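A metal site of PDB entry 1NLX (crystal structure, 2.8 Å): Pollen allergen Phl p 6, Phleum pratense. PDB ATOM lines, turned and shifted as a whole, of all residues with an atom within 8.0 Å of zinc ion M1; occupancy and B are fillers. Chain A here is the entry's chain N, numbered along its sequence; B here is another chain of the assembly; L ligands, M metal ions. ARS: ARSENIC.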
ATOM      1  N   LEU A  89     -18.299   5.631  -0.345  1.00  0.00           N
ATOM      2  CA  LEU A  89     -17.490   4.504   0.060  1.00  0.00           C
ATOM      3  C   LEU A  89     -17.935   3.214  -0.613  1.00  0.00           C
ATOM      4  O   LEU A  89     -17.127   2.521  -1.223  1.00  0.00           O
ATOM      5  CB  LEU A  89     -17.544   4.334   1.574  1.00  0.00           C
ATOM      6  CG  LEU A  89     -16.782   3.116   2.111  1.00  0.00           C
ATOM      7  CD1 LEU A  89     -15.330   3.187   1.686  1.00  0.00           C
ATOM      8  CD2 LEU A  89     -16.896   3.051   3.631  1.00  0.00           C
ATOM      9  N   HIS A  90     -19.217   2.894  -0.501  1.00  0.00           N
ATOM     10  CA  HIS A  90     -19.718   1.677  -1.102  1.00  0.00           C
ATOM     11  C   HIS A  90     -19.710   1.648  -2.626  1.00  0.00           C
ATOM     12  O   HIS A  90     -19.525   0.603  -3.232  1.00  0.00           O
ATOM     13  CB  HIS A  90     -21.111   1.361  -0.557  1.00  0.00           C
ATOM     14  CG  HIS A  90     -21.092   0.845   0.845  1.00  0.00           C
ATOM     15  ND1 HIS A  90     -20.980   1.666   1.944  1.00  0.00           N
ATOM     16  CD2 HIS A  90     -21.092  -0.426   1.333  1.00  0.00           C
ATOM     17  CE1 HIS A  90     -20.902   0.938   3.034  1.00  0.00           C
ATOM     18  NE2 HIS A  90     -20.963  -0.333   2.695  1.00  0.00           N
ATOM     19  N   SER A  92     -17.546   3.314  -4.690  1.00  0.00           N
ATOM     20  CA  SER A  92     -16.181   3.191  -5.136  1.00  0.00           C
ATOM     21  C   SER A  92     -15.670   1.747  -5.073  1.00  0.00           C
ATOM     22  O   SER A  92     -15.077   1.247  -6.034  1.00  0.00           O
ATOM     23  CB  SER A  92     -15.291   4.124  -4.306  1.00  0.00           C
ATOM     24  OG  SER A  92     -14.874   3.522  -3.088  1.00  0.00           O
ATOM     25  N   GLU A  93     -15.900   1.061  -3.951  1.00  0.00           N
ATOM     26  CA  GLU A  93     -15.453  -0.314  -3.784  1.00  0.00           C
ATOM     27  C   GLU A  93     -16.196  -1.291  -4.682  1.00  0.00           C
ATOM     28  O   GLU A  93     -15.573  -2.114  -5.361  1.00  0.00           O
ATOM     29  CB  GLU A  93     -15.560  -0.744  -2.315  1.00  0.00           C
ATOM     30  CG  GLU A  93     -14.515  -0.047  -1.440  1.00  0.00           C
ATOM     31  CD  GLU A  93     -14.408  -0.561  -0.003  1.00  0.00           C
ATOM     32  OE1 GLU A  93     -13.471  -0.101   0.681  1.00  0.00           O
ATOM     33  OE2 GLU A  93     -15.249  -1.385   0.436  1.00  0.00           O
ATOM     34  N   ARG A  96     -14.868  -1.158  -8.104  1.00  0.00           N
ATOM     35  CA  ARG A  96     -13.555  -1.793  -8.202  1.00  0.00           C
ATOM     36  C   ARG A  96     -13.712  -3.314  -8.273  1.00  0.00           C
ATOM     37  O   ARG A  96     -13.005  -3.985  -9.015  1.00  0.00           O
ATOM     38  CB  ARG A  96     -12.698  -1.415  -7.007  1.00  0.00           C
ATOM     39  CG  ARG A  96     -11.896  -0.157  -7.232  1.00  0.00           C
ATOM     40  CD  ARG A  96     -11.295   0.335  -5.958  1.00  0.00           C
ATOM     41  NE  ARG A  96     -11.329   1.791  -5.926  1.00  0.00           N
ATOM     42  CZ  ARG A  96     -11.548   2.492  -4.816  1.00  0.00           C
ATOM     43  NH1 ARG A  96     -11.567   3.829  -4.858  1.00  0.00           N
ATOM     44  NH2 ARG A  96     -11.753   1.863  -3.667  1.00  0.00           N
ATOM     45  N   VAL A 104      -9.384  -3.286  -3.472  1.00  0.00           N
ATOM     46  CA  VAL A 104     -10.652  -2.584  -3.444  1.00  0.00           C
ATOM     47  C   VAL A 104     -10.777  -1.576  -2.310  1.00  0.00           C
ATOM     48  O   VAL A 104     -11.692  -0.757  -2.332  1.00  0.00           O
ATOM     49  CB  VAL A 104     -11.876  -3.562  -3.430  1.00  0.00           C
ATOM     50  CG1 VAL A 104     -11.424  -4.978  -3.666  1.00  0.00           C
ATOM     51  CG2 VAL A 104     -12.646  -3.450  -2.144  1.00  0.00           C
ATOM     52  N   HIS A 105      -9.864  -1.590  -1.352  1.00  0.00           N
ATOM     53  CA  HIS A 105      -9.994  -0.634  -0.265  1.00  0.00           C
ATOM     54  C   HIS A 105      -9.288   0.724  -0.381  1.00  0.00           C
ATOM     55  O   HIS A 105      -9.953   1.738  -0.604  1.00  0.00           O
ATOM     56  CB  HIS A 105      -9.605  -1.269   1.067  1.00  0.00           C
ATOM     57  CG  HIS A 105      -9.989  -0.445   2.246  1.00  0.00           C
ATOM     58  ND1 HIS A 105     -11.301  -0.298   2.659  1.00  0.00           N
ATOM     59  CD2 HIS A 105      -9.250   0.337   3.074  1.00  0.00           C
ATOM     60  CE1 HIS A 105     -11.348   0.531   3.687  1.00  0.00           C
ATOM     61  NE2 HIS A 105     -10.116   0.920   3.961  1.00  0.00           N
ATOM     62  N   ALA A 106      -7.966   0.794  -0.214  1.00  0.00           N
ATOM     63  CA  ALA A 106      -7.312   2.108  -0.290  1.00  0.00           C
ATOM     64  C   ALA A 106      -5.783   2.196  -0.408  1.00  0.00           C
ATOM     65  O   ALA A 106      -5.069   1.182  -0.456  1.00  0.00           O
ATOM     66  CB  ALA A 106      -7.793   2.965   0.884  1.00  0.00           C
ATOM     67  N   ALA B  70     -10.124  -8.924  -2.505  1.00  0.00           N
ATOM     68  CA  ALA B  70     -10.666  -7.776  -1.800  1.00  0.00           C
ATOM     69  C   ALA B  70     -10.400  -7.952  -0.320  1.00  0.00           C
ATOM     70  O   ALA B  70      -9.850  -7.062   0.331  1.00  0.00           O
ATOM     71  CB  ALA B  70     -12.159  -7.682  -2.053  1.00  0.00           C
ATOM     72  N   ALA B  74      -7.582  -5.992   2.075  1.00  0.00           N
ATOM     73  CA  ALA B  74      -8.062  -5.071   3.075  1.00  0.00           C
ATOM     74  C   ALA B  74      -7.351  -5.380   4.396  1.00  0.00           C
ATOM     75  O   ALA B  74      -6.854  -4.464   5.072  1.00  0.00           O
ATOM     76  CB  ALA B  74      -9.562  -5.213   3.228  1.00  0.00           C
ATOM     77  N   ALA B  86     -11.470  -6.485   9.211  1.00  0.00           N
ATOM     78  CA  ALA B  86     -11.299  -5.918   7.875  1.00  0.00           C
ATOM     79  C   ALA B  86     -11.599  -6.957   6.802  1.00  0.00           C
ATOM     80  O   ALA B  86     -12.265  -6.671   5.808  1.00  0.00           O
ATOM     81  CB  ALA B  86      -9.900  -5.406   7.702  1.00  0.00           C
ATOM     82  N   LEU B  89     -15.533  -8.118   6.917  1.00  0.00           N
ATOM     83  CA  LEU B  89     -16.368  -7.058   6.382  1.00  0.00           C
ATOM     84  C   LEU B  89     -16.275  -6.981   4.865  1.00  0.00           C
ATOM     85  O   LEU B  89     -17.300  -7.000   4.180  1.00  0.00           O
ATOM     86  CB  LEU B  89     -15.967  -5.715   6.986  1.00  0.00           C
ATOM     87  CG  LEU B  89     -16.706  -4.499   6.410  1.00  0.00           C
ATOM     88  CD1 LEU B  89     -18.204  -4.693   6.592  1.00  0.00           C
ATOM     89  CD2 LEU B  89     -16.217  -3.236   7.099  1.00  0.00           C
ATOM     90  N   HIS B  90     -15.059  -6.881   4.337  1.00  0.00           N
ATOM     91  CA  HIS B  90     -14.886  -6.786   2.902  1.00  0.00           C
ATOM     92  C   HIS B  90     -15.257  -8.052   2.136  1.00  0.00           C
ATOM     93  O   HIS B  90     -15.716  -7.977   0.993  1.00  0.00           O
ATOM     94  CB  HIS B  90     -13.473  -6.366   2.571  1.00  0.00           C
ATOM     95  CG  HIS B  90     -13.223  -4.918   2.845  1.00  0.00           C
ATOM     96  ND1 HIS B  90     -12.971  -4.435   4.109  1.00  0.00           N
ATOM     97  CD2 HIS B  90     -13.281  -3.833   2.028  1.00  0.00           C
ATOM     98  CE1 HIS B  90     -12.889  -3.120   4.059  1.00  0.00           C
ATOM     99  NE2 HIS B  90     -13.066  -2.726   2.815  1.00  0.00           N
ATOM    100  N   GLU B  93     -19.263  -8.379   1.930  1.00  0.00           N
ATOM    101  CA  GLU B  93     -19.835  -7.434   0.973  1.00  0.00           C
ATOM    102  C   GLU B  93     -19.467  -7.793  -0.461  1.00  0.00           C
ATOM    103  O   GLU B  93     -20.342  -7.860  -1.341  1.00  0.00           O
ATOM    104  CB  GLU B  93     -19.415  -5.996   1.299  1.00  0.00           C
ATOM    105  CG  GLU B  93     -20.144  -5.475   2.542  1.00  0.00           C
ATOM    106  CD  GLU B  93     -19.969  -3.971   2.827  1.00  0.00           C
ATOM    107  OE1 GLU B  93     -20.619  -3.511   3.793  1.00  0.00           O
ATOM    108  OE2 GLU B  93     -19.205  -3.262   2.126  1.00  0.00           O
HETATM  109 AS   ARS L   1     -16.903  -0.963   3.994  1.00  0.00          AS
HETATM  110 ZN    ZN M   1     -13.492  -0.678   2.797  1.00  0.00          ZN
HETATM  111 ZN    ZN M   2     -20.297  -1.470   4.445  1.00  0.00          ZN
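Zinc ion M1 is bound by NE2 of His 90 of chain B (2.1 Å), OE1 of Glu 93 of chain A (2.2 Å) and ND1 of His 105 (2.2 Å).
Zinc ion M1 has three donor atoms within binding distance.
Within 4 Å of zinc ion M1: Glu 93 of chain A, His 105 and His 90 of chain B.
A ring nitrogen (ND1) of His 90 of chain B is in hydrogen-bond range of the backbone carbonyl oxygen (O) of Ala 86 of chain B.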
